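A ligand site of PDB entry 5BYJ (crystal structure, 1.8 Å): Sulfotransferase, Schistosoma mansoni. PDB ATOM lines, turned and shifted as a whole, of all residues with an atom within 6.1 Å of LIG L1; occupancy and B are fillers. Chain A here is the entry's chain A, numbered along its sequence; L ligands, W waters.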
ATOM      1  N   LEU A  17     -29.944 -12.501   7.789  1.00  0.00           N
ATOM      2  CA  LEU A  17     -28.814 -11.982   7.020  1.00  0.00           C
ATOM      3  C   LEU A  17     -27.846 -11.237   7.927  1.00  0.00           C
ATOM      4  O   LEU A  17     -28.206 -10.843   9.022  1.00  0.00           O
ATOM      5  CB  LEU A  17     -29.326 -11.057   5.906  1.00  0.00           C
ATOM      6  CG  LEU A  17     -30.152 -11.746   4.820  1.00  0.00           C
ATOM      7  CD1 LEU A  17     -30.880 -10.692   3.997  1.00  0.00           C
ATOM      8  CD2 LEU A  17     -29.241 -12.575   3.934  1.00  0.00           C
ATOM      9  N   PRO A  18     -26.591 -11.038   7.463  1.00  0.00           N
ATOM     10  CA  PRO A  18     -25.670 -10.259   8.294  1.00  0.00           C
ATOM     11  C   PRO A  18     -26.222  -8.860   8.613  1.00  0.00           C
ATOM     12  O   PRO A  18     -27.000  -8.340   7.817  1.00  0.00           O
ATOM     13  CB  PRO A  18     -24.409 -10.150   7.423  1.00  0.00           C
ATOM     14  CG  PRO A  18     -24.819 -10.602   6.063  1.00  0.00           C
ATOM     15  CD  PRO A  18     -25.951 -11.546   6.243  1.00  0.00           C
ATOM     16  N   ARG A  19     -25.810  -8.299   9.752  1.00  0.00           N
ATOM     17  CA  ARG A  19     -26.234  -6.979  10.247  1.00  0.00           C
ATOM     18  C   ARG A  19     -27.703  -6.951  10.693  1.00  0.00           C
ATOM     19  O   ARG A  19     -28.334  -5.891  10.682  1.00  0.00           O
ATOM     20  CB  ARG A  19     -25.966  -5.869   9.208  1.00  0.00           C
ATOM     21  CG  ARG A  19     -24.540  -5.839   8.660  1.00  0.00           C
ATOM     22  CD  ARG A  19     -23.485  -5.966   9.778  1.00  0.00           C
ATOM     23  NE  ARG A  19     -23.481  -4.820  10.682  1.00  0.00           N
ATOM     24  CZ  ARG A  19     -22.748  -4.741  11.787  1.00  0.00           C
ATOM     25  NH1 ARG A  19     -21.957  -5.747  12.141  1.00  0.00           N
ATOM     26  NH2 ARG A  19     -22.801  -3.663  12.557  1.00  0.00           N
ATOM     27  N   THR A  20     -28.237  -8.099  11.117  1.00  0.00           N
ATOM     28  CA  THR A  20     -29.599  -8.178  11.665  1.00  0.00           C
ATOM     29  C   THR A  20     -29.623  -8.674  13.109  1.00  0.00           C
ATOM     30  O   THR A  20     -30.674  -9.062  13.613  1.00  0.00           O
ATOM     31  CB  THR A  20     -30.515  -9.098  10.824  1.00  0.00           C
ATOM     32  OG1 THR A  20     -29.994 -10.442  10.818  1.00  0.00           O
ATOM     33  CG2 THR A  20     -30.584  -8.594   9.388  1.00  0.00           C
ATOM     34  N   GLY A  21     -28.485  -8.632  13.785  1.00  0.00           N
ATOM     35  CA  GLY A  21     -28.406  -9.077  15.167  1.00  0.00           C
ATOM     36  C   GLY A  21     -27.863 -10.491  15.328  1.00  0.00           C
ATOM     37  O   GLY A  21     -28.128 -11.160  16.345  1.00  0.00           O
ATOM     38  N   THR A  22     -27.091 -10.958  14.348  1.00  0.00           N
ATOM     39  CA  THR A  22     -26.634 -12.350  14.374  1.00  0.00           C
ATOM     40  C   THR A  22     -25.606 -12.597  15.457  1.00  0.00           C
ATOM     41  O   THR A  22     -25.589 -13.661  16.074  1.00  0.00           O
ATOM     42  CB  THR A  22     -26.058 -12.787  12.992  1.00  0.00           C
ATOM     43  OG1 THR A  22     -24.903 -11.994  12.677  1.00  0.00           O
ATOM     44  CG2 THR A  22     -27.097 -12.591  11.915  1.00  0.00           C
ATOM     45  N   LYS A  23     -24.727 -11.627  15.717  1.00  0.00           N
ATOM     46  CA  LYS A  23     -23.689 -11.877  16.717  1.00  0.00           C
ATOM     47  C   LYS A  23     -24.292 -11.878  18.126  1.00  0.00           C
ATOM     48  O   LYS A  23     -23.903 -12.675  18.976  1.00  0.00           O
ATOM     49  CB  LYS A  23     -22.565 -10.855  16.597  1.00  0.00           C
ATOM     50  CG  LYS A  23     -21.383 -11.091  17.566  1.00  0.00           C
ATOM     51  CD  LYS A  23     -20.805 -12.491  17.439  1.00  0.00           C
ATOM     52  CE  LYS A  23     -19.420 -12.614  18.063  1.00  0.00           C
ATOM     53  NZ  LYS A  23     -19.397 -12.548  19.545  1.00  0.00           N
ATOM     54  N   SER A  24     -25.243 -10.984  18.372  1.00  0.00           N
ATOM     55  CA  SER A  24     -25.957 -10.995  19.651  1.00  0.00           C
ATOM     56  C   SER A  24     -26.687 -12.326  19.814  1.00  0.00           C
ATOM     57  O   SER A  24     -26.676 -12.913  20.892  1.00  0.00           O
ATOM     58  CB  SER A  24     -26.938  -9.826  19.743  1.00  0.00           C
ATOM     59  OG  SER A  24     -26.208  -8.611  19.812  1.00  0.00           O
ATOM     60  N   HIS A  39     -20.851 -18.803  13.233  1.00  0.00           N
ATOM     61  CA  HIS A  39     -21.018 -17.395  12.867  1.00  0.00           C
ATOM     62  C   HIS A  39     -19.816 -17.042  12.001  1.00  0.00           C
ATOM     63  O   HIS A  39     -18.816 -17.742  12.075  1.00  0.00           O
ATOM     64  CB  HIS A  39     -21.064 -16.510  14.123  1.00  0.00           C
ATOM     65  CG  HIS A  39     -21.403 -15.064  13.849  1.00  0.00           C
ATOM     66  ND1 HIS A  39     -20.441 -14.118  13.547  1.00  0.00           N
ATOM     67  CD2 HIS A  39     -22.582 -14.411  13.856  1.00  0.00           C
ATOM     68  CE1 HIS A  39     -21.035 -12.952  13.364  1.00  0.00           C
ATOM     69  NE2 HIS A  39     -22.329 -13.104  13.547  1.00  0.00           N
ATOM     70  N   ASP A  93     -25.709 -16.260  10.506  1.00  0.00           N
ATOM     71  CA  ASP A  93     -24.857 -15.380   9.684  1.00  0.00           C
ATOM     72  C   ASP A  93     -24.405 -16.075   8.396  1.00  0.00           C
ATOM     73  O   ASP A  93     -24.686 -17.266   8.181  1.00  0.00           O
ATOM     74  CB  ASP A  93     -23.647 -14.918  10.511  1.00  0.00           C
ATOM     75  CG  ASP A  93     -22.943 -13.703   9.951  1.00  0.00           C
ATOM     76  OD1 ASP A  93     -23.526 -12.981   9.117  1.00  0.00           O
ATOM     77  OD2 ASP A  93     -21.780 -13.464  10.355  1.00  0.00           O
ATOM     78  N   ARG A 117     -34.861  -6.524  10.560  1.00  0.00           N
ATOM     79  CA  ARG A 117     -34.857  -5.139  11.014  1.00  0.00           C
ATOM     80  C   ARG A 117     -35.263  -4.237   9.845  1.00  0.00           C
ATOM     81  O   ARG A 117     -35.453  -4.706   8.707  1.00  0.00           O
ATOM     82  CB  ARG A 117     -33.482  -4.724  11.530  1.00  0.00           C
ATOM     83  CG  ARG A 117     -32.462  -4.574  10.403  1.00  0.00           C
ATOM     84  CD  ARG A 117     -31.044  -4.363  10.928  1.00  0.00           C
ATOM     85  NE  ARG A 117     -30.876  -3.102  11.654  1.00  0.00           N
ATOM     86  CZ  ARG A 117     -29.696  -2.628  12.030  1.00  0.00           C
ATOM     87  NH1 ARG A 117     -28.583  -3.291  11.711  1.00  0.00           N
ATOM     88  NH2 ARG A 117     -29.607  -1.482  12.685  1.00  0.00           N
ATOM     89  N   ASP A 121     -31.921   0.716   7.777  1.00  0.00           N
ATOM     90  CA  ASP A 121     -30.963   0.560   8.865  1.00  0.00           C
ATOM     91  C   ASP A 121     -30.011  -0.589   8.533  1.00  0.00           C
ATOM     92  O   ASP A 121     -28.817  -0.519   8.833  1.00  0.00           O
ATOM     93  CB  ASP A 121     -31.648   0.272  10.199  1.00  0.00           C
ATOM     94  CG  ASP A 121     -32.349   1.487  10.795  1.00  0.00           C
ATOM     95  OD1 ASP A 121     -32.100   2.633  10.346  1.00  0.00           O
ATOM     96  OD2 ASP A 121     -33.142   1.281  11.739  1.00  0.00           O
ATOM     97  N   HIS A 124     -27.544   0.566   5.699  1.00  0.00           N
ATOM     98  CA  HIS A 124     -26.568   1.487   6.258  1.00  0.00           C
ATOM     99  C   HIS A 124     -25.499   0.731   7.040  1.00  0.00           C
ATOM    100  O   HIS A 124     -24.301   1.003   6.896  1.00  0.00           O
ATOM    101  CB  HIS A 124     -27.259   2.521   7.152  1.00  0.00           C
ATOM    102  CG  HIS A 124     -26.333   3.437   7.872  1.00  0.00           C
ATOM    103  ND1 HIS A 124     -26.074   3.326   9.222  1.00  0.00           N
ATOM    104  CD2 HIS A 124     -25.602   4.488   7.434  1.00  0.00           C
ATOM    105  CE1 HIS A 124     -25.215   4.274   9.582  1.00  0.00           C
ATOM    106  NE2 HIS A 124     -24.916   4.989   8.516  1.00  0.00           N
ATOM    107  N   SER A 125     -25.941  -0.220   7.853  1.00  0.00           N
ATOM    108  CA  SER A 125     -25.054  -1.050   8.643  1.00  0.00           C
ATOM    109  C   SER A 125     -24.162  -1.922   7.743  1.00  0.00           C
ATOM    110  O   SER A 125     -22.953  -2.027   7.962  1.00  0.00           O
ATOM    111  CB  SER A 125     -25.873  -1.949   9.589  1.00  0.00           C
ATOM    112  OG  SER A 125     -25.037  -2.596  10.523  1.00  0.00           O
ATOM    113  N   LEU A 126     -24.764  -2.530   6.731  1.00  0.00           N
ATOM    114  CA  LEU A 126     -24.022  -3.362   5.771  1.00  0.00           C
ATOM    115  C   LEU A 126     -22.896  -2.566   5.079  1.00  0.00           C
ATOM    116  O   LEU A 126     -21.777  -3.071   4.924  1.00  0.00           O
ATOM    117  CB  LEU A 126     -24.997  -3.924   4.727  1.00  0.00           C
ATOM    118  CG  LEU A 126     -24.470  -5.077   3.876  1.00  0.00           C
ATOM    119  CD1 LEU A 126     -24.561  -6.383   4.650  1.00  0.00           C
ATOM    120  CD2 LEU A 126     -25.264  -5.152   2.568  1.00  0.00           C
ATOM    121  N   VAL A 129     -19.773  -1.985   7.307  1.00  0.00           N
ATOM    122  CA  VAL A 129     -19.060  -3.136   7.863  1.00  0.00           C
ATOM    123  C   VAL A 129     -18.727  -4.248   6.858  1.00  0.00           C
ATOM    124  O   VAL A 129     -17.606  -4.749   6.839  1.00  0.00           O
ATOM    125  CB  VAL A 129     -19.876  -3.752   9.006  1.00  0.00           C
ATOM    126  CG1 VAL A 129     -19.185  -5.002   9.587  1.00  0.00           C
ATOM    127  CG2 VAL A 129     -20.125  -2.704  10.095  1.00  0.00           C
ATOM    128  N   LEU A 205     -35.041  -6.961  15.727  1.00  0.00           N
ATOM    129  CA  LEU A 205     -33.994  -6.438  16.591  1.00  0.00           C
ATOM    130  C   LEU A 205     -34.623  -5.783  17.797  1.00  0.00           C
ATOM    131  O   LEU A 205     -35.553  -5.001  17.661  1.00  0.00           O
ATOM    132  CB  LEU A 205     -33.155  -5.398  15.848  1.00  0.00           C
ATOM    133  CG  LEU A 205     -31.880  -5.902  15.178  1.00  0.00           C
ATOM    134  CD1 LEU A 205     -31.082  -4.740  14.620  1.00  0.00           C
ATOM    135  CD2 LEU A 205     -31.057  -6.720  16.152  1.00  0.00           C
ATOM    136  N   GLY A 206     -34.120  -6.101  18.981  1.00  0.00           N
ATOM    137  CA  GLY A 206     -34.634  -5.528  20.210  1.00  0.00           C
ATOM    138  C   GLY A 206     -35.623  -6.393  20.960  1.00  0.00           C
ATOM    139  O   GLY A 206     -36.009  -6.066  22.096  1.00  0.00           O
ATOM    140  N   TYR A 226     -30.028  -9.547  27.528  1.00  0.00           N
ATOM    141  CA  TYR A 226     -29.853 -10.072  26.166  1.00  0.00           C
ATOM    142  C   TYR A 226     -28.696  -9.339  25.486  1.00  0.00           C
ATOM    143  O   TYR A 226     -28.584  -8.112  25.603  1.00  0.00           O
ATOM    144  CB  TYR A 226     -31.139  -9.920  25.359  1.00  0.00           C
ATOM    145  CG  TYR A 226     -31.058 -10.580  24.012  1.00  0.00           C
ATOM    146  CD1 TYR A 226     -31.401 -11.923  23.849  1.00  0.00           C
ATOM    147  CD2 TYR A 226     -30.618  -9.878  22.903  1.00  0.00           C
ATOM    148  CE1 TYR A 226     -31.312 -12.546  22.610  1.00  0.00           C
ATOM    149  CE2 TYR A 226     -30.526 -10.479  21.662  1.00  0.00           C
ATOM    150  CZ  TYR A 226     -30.876 -11.810  21.518  1.00  0.00           C
ATOM    151  OH  TYR A 226     -30.785 -12.397  20.279  1.00  0.00           O
ATOM    152  N   PRO A 227     -27.817 -10.074  24.789  1.00  0.00           N
ATOM    153  CA  PRO A 227     -26.636  -9.434  24.186  1.00  0.00           C
ATOM    154  C   PRO A 227     -26.962  -8.255  23.281  1.00  0.00           C
ATOM    155  O   PRO A 227     -27.959  -8.271  22.538  1.00  0.00           O
ATOM    156  CB  PRO A 227     -25.999 -10.581  23.391  1.00  0.00           C
ATOM    157  CG  PRO A 227     -26.357 -11.793  24.192  1.00  0.00           C
ATOM    158  CD  PRO A 227     -27.760 -11.540  24.686  1.00  0.00           C
ATOM    159  N   CYS A 228     -26.151  -7.222  23.382  1.00  0.00           N
ATOM    160  CA  CYS A 228     -26.226  -6.102  22.449  1.00  0.00           C
ATOM    161  C   CYS A 228     -24.818  -5.775  21.976  1.00  0.00           C
ATOM    162  O   CYS A 228     -24.153  -4.923  22.552  1.00  0.00           O
ATOM    163  CB  CYS A 228     -26.885  -4.889  23.101  1.00  0.00           C
ATOM    164  SG  CYS A 228     -27.198  -3.560  21.943  1.00  0.00           S
ATOM    165  N   VAL A 229     -24.355  -6.482  20.954  1.00  0.00           N
ATOM    166  CA  VAL A 229     -22.976  -6.346  20.482  1.00  0.00           C
ATOM    167  C   VAL A 229     -22.909  -6.154  18.981  1.00  0.00           C
ATOM    168  O   VAL A 229     -23.905  -6.312  18.282  1.00  0.00           O
ATOM    169  CB  VAL A 229     -22.122  -7.572  20.868  1.00  0.00           C
ATOM    170  CG1 VAL A 229     -22.059  -7.727  22.374  1.00  0.00           C
ATOM    171  CG2 VAL A 229     -22.690  -8.835  20.228  1.00  0.00           C
ATOM    172  N   ASN A 230     -21.715  -5.794  18.494  1.00  0.00           N
ATOM    173  CA  ASN A 230     -21.404  -5.777  17.067  1.00  0.00           C
ATOM    174  C   ASN A 230     -22.064  -4.614  16.309  1.00  0.00           C
ATOM    175  O   ASN A 230     -22.401  -4.744  15.133  1.00  0.00           O
ATOM    176  CB  ASN A 230     -21.764  -7.128  16.418  1.00  0.00           C
ATOM    177  CG  ASN A 230     -20.929  -7.430  15.173  1.00  0.00           C
ATOM    178  OD1 ASN A 230     -19.861  -6.867  14.988  1.00  0.00           O
ATOM    179  ND2 ASN A 230     -21.445  -8.299  14.311  1.00  0.00           N
ATOM    180  N   SER A 231     -22.248  -3.470  16.992  1.00  0.00           N
ATOM    181  CA  SER A 231     -22.710  -2.253  16.326  1.00  0.00           C
ATOM    182  C   SER A 231     -21.675  -1.785  15.314  1.00  0.00           C
ATOM    183  O   SER A 231     -20.489  -2.049  15.468  1.00  0.00           O
ATOM    184  CB  SER A 231     -22.963  -1.123  17.335  1.00  0.00           C
ATOM    185  OG  SER A 231     -21.736  -0.684  17.911  1.00  0.00           O
ATOM    186  N   HIS A 232     -22.104  -1.061  14.279  1.00  0.00           N
ATOM    187  CA  HIS A 232     -21.119  -0.612  13.303  1.00  0.00           C
ATOM    188  C   HIS A 232     -20.125   0.357  13.951  1.00  0.00           C
ATOM    189  O   HIS A 232     -18.943   0.356  13.582  1.00  0.00           O
ATOM    190  CB  HIS A 232     -21.784   0.024  12.066  1.00  0.00           C
ATOM    191  CG  HIS A 232     -22.488   1.322  12.307  1.00  0.00           C
ATOM    192  ND1 HIS A 232     -21.827   2.533  12.389  1.00  0.00           N
ATOM    193  CD2 HIS A 232     -23.807   1.604  12.439  1.00  0.00           C
ATOM    194  CE1 HIS A 232     -22.706   3.500  12.584  1.00  0.00           C
ATOM    195  NE2 HIS A 232     -23.914   2.969  12.613  1.00  0.00           N
ATOM    196  N   HIS A 233     -20.578   1.120  14.943  1.00  0.00           N
ATOM    197  CA  HIS A 233     -19.678   2.017  15.670  1.00  0.00           C
ATOM    198  C   HIS A 233     -18.549   1.229  16.306  1.00  0.00           C
ATOM    199  O   HIS A 233     -17.376   1.624  16.248  1.00  0.00           O
ATOM    200  CB  HIS A 233     -20.408   2.814  16.745  1.00  0.00           C
ATOM    201  CG  HIS A 233     -21.398   3.805  16.213  1.00  0.00           C
ATOM    202  ND1 HIS A 233     -21.017   4.940  15.528  1.00  0.00           N
ATOM    203  CD2 HIS A 233     -22.741   3.853  16.304  1.00  0.00           C
ATOM    204  CE1 HIS A 233     -22.091   5.635  15.208  1.00  0.00           C
ATOM    205  NE2 HIS A 233     -23.157   4.993  15.663  1.00  0.00           N
HETATM  206  P1  LIG L   1     -25.894  -1.348  13.620  1.00  0.00           P
HETATM  207  O1  LIG L   1     -26.960  -0.508  12.964  1.00  0.00           O
HETATM  208  O2  LIG L   1     -24.693  -1.563  12.705  1.00  0.00           O
HETATM  209  O3  LIG L   1     -25.410  -0.743  14.919  1.00  0.00           O
HETATM  210  P2  LIG L   1     -24.820  -8.551  13.170  1.00  0.00           P
HETATM  211  O4  LIG L   1     -25.784  -9.491  12.489  1.00  0.00           O
HETATM  212  O5  LIG L   1     -24.270  -9.105  14.446  1.00  0.00           O
HETATM  213  O6  LIG L   1     -23.728  -8.078  12.227  1.00  0.00           O
HETATM  214  O7  LIG L   1     -25.776  -7.320  13.521  1.00  0.00           O
HETATM  215  C1  LIG L   1     -25.267  -6.180  14.225  1.00  0.00           C
HETATM  216  C2  LIG L   1     -26.319  -5.103  14.192  1.00  0.00           C
HETATM  217  O8  LIG L   1     -27.428  -5.455  15.077  1.00  0.00           O
HETATM  218  C3  LIG L   1     -25.805  -3.792  14.687  1.00  0.00           C
HETATM  219  O9  LIG L   1     -26.565  -2.755  14.023  1.00  0.00           O
HETATM  220  C4  LIG L   1     -26.140  -3.850  16.130  1.00  0.00           C
HETATM  221  O10 LIG L   1     -26.168  -2.561  16.729  1.00  0.00           O
HETATM  222  C5  LIG L   1     -27.503  -4.453  16.122  1.00  0.00           C
HETATM  223  N1  LIG L   1     -27.854  -5.107  17.328  1.00  0.00           N
HETATM  224  C6  LIG L   1     -27.265  -6.194  17.831  1.00  0.00           C
HETATM  225  N2  LIG L   1     -27.841  -6.545  18.980  1.00  0.00           N
HETATM  226  C7  LIG L   1     -28.849  -5.652  19.231  1.00  0.00           C
HETATM  227  C8  LIG L   1     -29.820  -5.497  20.271  1.00  0.00           C
HETATM  228  N3  LIG L   1     -29.864  -6.392  21.352  1.00  0.00           N
HETATM  229  N4  LIG L   1     -30.686  -4.472  20.198  1.00  0.00           N
HETATM  230  C9  LIG L   1     -30.658  -3.630  19.177  1.00  0.00           C
HETATM  231  N5  LIG L   1     -29.769  -3.729  18.187  1.00  0.00           N
HETATM  232  C10 LIG L   1     -28.855  -4.730  18.176  1.00  0.00           C
HETATM  233  C1  LG2 L   2     -14.753  -9.493  10.792  1.00  0.00           C
HETATM  234  C2  LG2 L   2     -16.250  -9.221  10.945  1.00  0.00           C
HETATM  235  C3  LG2 L   2     -16.930  -9.499   9.755  1.00  0.00           C
HETATM  236  C4  LG2 L   2     -18.248  -9.992   9.780  1.00  0.00           C
HETATM  237  C5  LG2 L   2     -18.950 -10.275   8.607  1.00  0.00           C
HETATM  238  C6  LG2 L   2     -20.267 -10.766   8.669  1.00  0.00           C
HETATM  239  O1  LG2 L   2     -20.583 -11.321   9.965  1.00  0.00           O
HETATM  240  C7  LG2 L   2     -18.276 -10.019   7.393  1.00  0.00           C
HETATM  241  N1  LG2 L   2     -18.835 -10.237   6.191  1.00  0.00           N
HETATM  242  O2  LG2 L   2     -18.295  -9.450   5.136  1.00  0.00           O
HETATM  243  O3  LG2 L   2     -19.849 -11.338   5.927  1.00  0.00           O
HETATM  244  C8  LG2 L   2     -16.983  -9.513   7.363  1.00  0.00           C
HETATM  245  C9  LG2 L   2     -16.308  -9.249   8.542  1.00  0.00           C
HETATM  246  N2  LG2 L   2     -14.984  -8.763   8.475  1.00  0.00           N
HETATM  247  C10 LG2 L   2     -14.183  -8.613   9.707  1.00  0.00           C
HETATM  248  C11 LG2 L   2     -14.219  -7.188  10.203  1.00  0.00           C
HETATM  249  N3  LG2 L   2     -13.396  -6.304   9.379  1.00  0.00           N
HETATM  250  C12 LG2 L   2     -12.364  -5.750  10.268  1.00  0.00           C
HETATM  251  C13 LG2 L   2     -12.994  -5.221  11.557  1.00  0.00           C
HETATM  252  C14 LG2 L   2     -11.568  -4.639   9.548  1.00  0.00           C
HETATM  253  O   HOH W   1     -30.164  -1.193  16.840  1.00  0.00           O
HETATM  254  O   HOH W   2     -25.324  -8.499  16.889  1.00  0.00           O
HETATM  255  O   HOH W   3     -20.866  -8.596  10.888  1.00  0.00           O
HETATM  256  O   HOH W   4     -27.666   1.039  10.935  1.00  0.00           O
HETATM  257  O   HOH W   5     -25.912  -1.927  19.570  1.00  0.00           O
HETATM  258  O   HOH W   6     -32.113  -3.432  22.325  1.00  0.00           O
HETATM  259  O   HOH W   7     -32.220  -6.781  23.438  1.00  0.00           O
HETATM  260  O   HOH W   8     -27.716   1.403  14.503  1.00  0.00           O
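OG of Ser 125 sits at hydrogen-bond distance from O2 of LIG L1, at 2.4 Å. N of Thr 22 sits at hydrogen-bond distance from O4 of LIG L1. O4 of LIG L1 lies within hydrogen-bond range of OG1 of Thr 22 (2.7 Å). N2 of LIG L1 lies within hydrogen-bond range of OG of Ser 24 (2.8 Å). An oxygen (O4) of LIG L1 lies within hydrogen-bond range of the backbone NH of Arg 19 (3.0 Å). The guanidinium group (NH2) of Arg 19 lies within salt-bridge range of an oxygen (O2) of LIG L1 (2.8 Å). O1 of LIG L1 is in salt-bridge range of NH2 of Arg 117, 2.8 Å away. The backbone NH (N) of Lys 23 sits at hydrogen-bond distance from an oxygen (O5) of LIG L1, 2.9 Å away. O of Pro 227 lies within hydrogen-bond range of N3 of LIG L1 (2.9 Å). O5 of LIG L1 sits at hydrogen-bond distance from ND2 of Asn 230, 2.9 Å away. N of Gly 21 lies within hydrogen-bond range of O7 of LIG L1 (3.0 Å). N of His 232 lies within hydrogen-bond range of O2 of LIG L1, at 3.1 Å. N of Thr 20 is in hydrogen-bond range of O4 of LIG L1, at 3.1 Å. An oxygen (O1) of LG2 L2 is in hydrogen-bond range of the side-chain carboxylate (OD2) of Asp 93 (2.5 Å).
Pro 18 touches LIG L1 (C to O4, 3.95 Å). Leu 205 touches LIG L1. Gly 206 touches LIG L1 (N to N4, 3.99 Å). CD2 of Tyr 226 touches N3 of LIG L1, at 3.9 Å. SG of Cys 228 touches C8 of LIG L1, at 3.7 Å. Val 229 touches LIG L1 (O to C6, 3.4 Å). CA of Ser 231 touches O3 of LIG L1, 3.4 Å away. Hydrophobic or aromatic side chains within 4 Å of LIG L1: Leu 205, Tyr 226 and His 232. 18 residues have an atom within 4 Å of LIG L1: Pro 18, Arg 19, Thr 20, Gly 21, Thr 22, Lys 23, Ser 24, Arg 117, Ser 125, Leu 205, Gly 206, Tyr 226, Pro 227, Cys 228, Val 229, Asn 230, Ser 231 and His 232. The nearest printed residue that does not touch LIG L1 is Leu 17 (4.4 Å).
Water W4 lies within hydrogen-bond range of an oxygen (O1) of LIG L1 (2.6 Å), the backbone carbonyl oxygen (O) of Asp 121 (2.9 Å) and a ring nitrogen (ND1) of His 124 (3.3 Å). Water W2 lies within hydrogen-bond range of an oxygen (O5) of LIG L1 (2.7 Å), the backbone NH of Ser 24 (2.9 Å), the backbone carbonyl oxygen of Val 229 (3.0 Å) and the backbone NH of Lys 23 (3.4 Å). Water W5 bridges O10 of LIG L1 and SG of Cys 228. Water W3 lies within hydrogen-bond range of O1 of LG2 L2 (2.9 Å), O6 of LIG L1 (3.2 Å), NH1 of Arg 19 (3.3 Å) and ND2 of Asn 230 (3.5 Å).
The side-chain hydroxyl of Ser 125 sits at hydrogen-bond distance from the guanidinium group of Arg 19, 2.7 Å away. OG1 of Thr 22 is in hydrogen-bond range of NE2 of His 39, at 2.9 Å. The backbone carbonyl oxygen (O) of Pro 227 is in hydrogen-bond range of the side-chain hydroxyl (OG) of Ser 24 (3.3 Å). The side-chain hydroxyl (OG) of Ser 24 lies within hydrogen-bond range of the backbone NH (N) of Val 229. The backbone carbonyl oxygen of Arg 19 is in hydrogen-bond range of the guanidinium group of Arg 117 (2.8 Å). The backbone carbonyl oxygen (O) of Asn 230 sits at hydrogen-bond distance from the guanidinium group (NH2) of Arg 19 (2.8 Å). The side-chain hydroxyl of Thr 20 lies within hydrogen-bond range of the backbone carbonyl oxygen of Leu 17.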
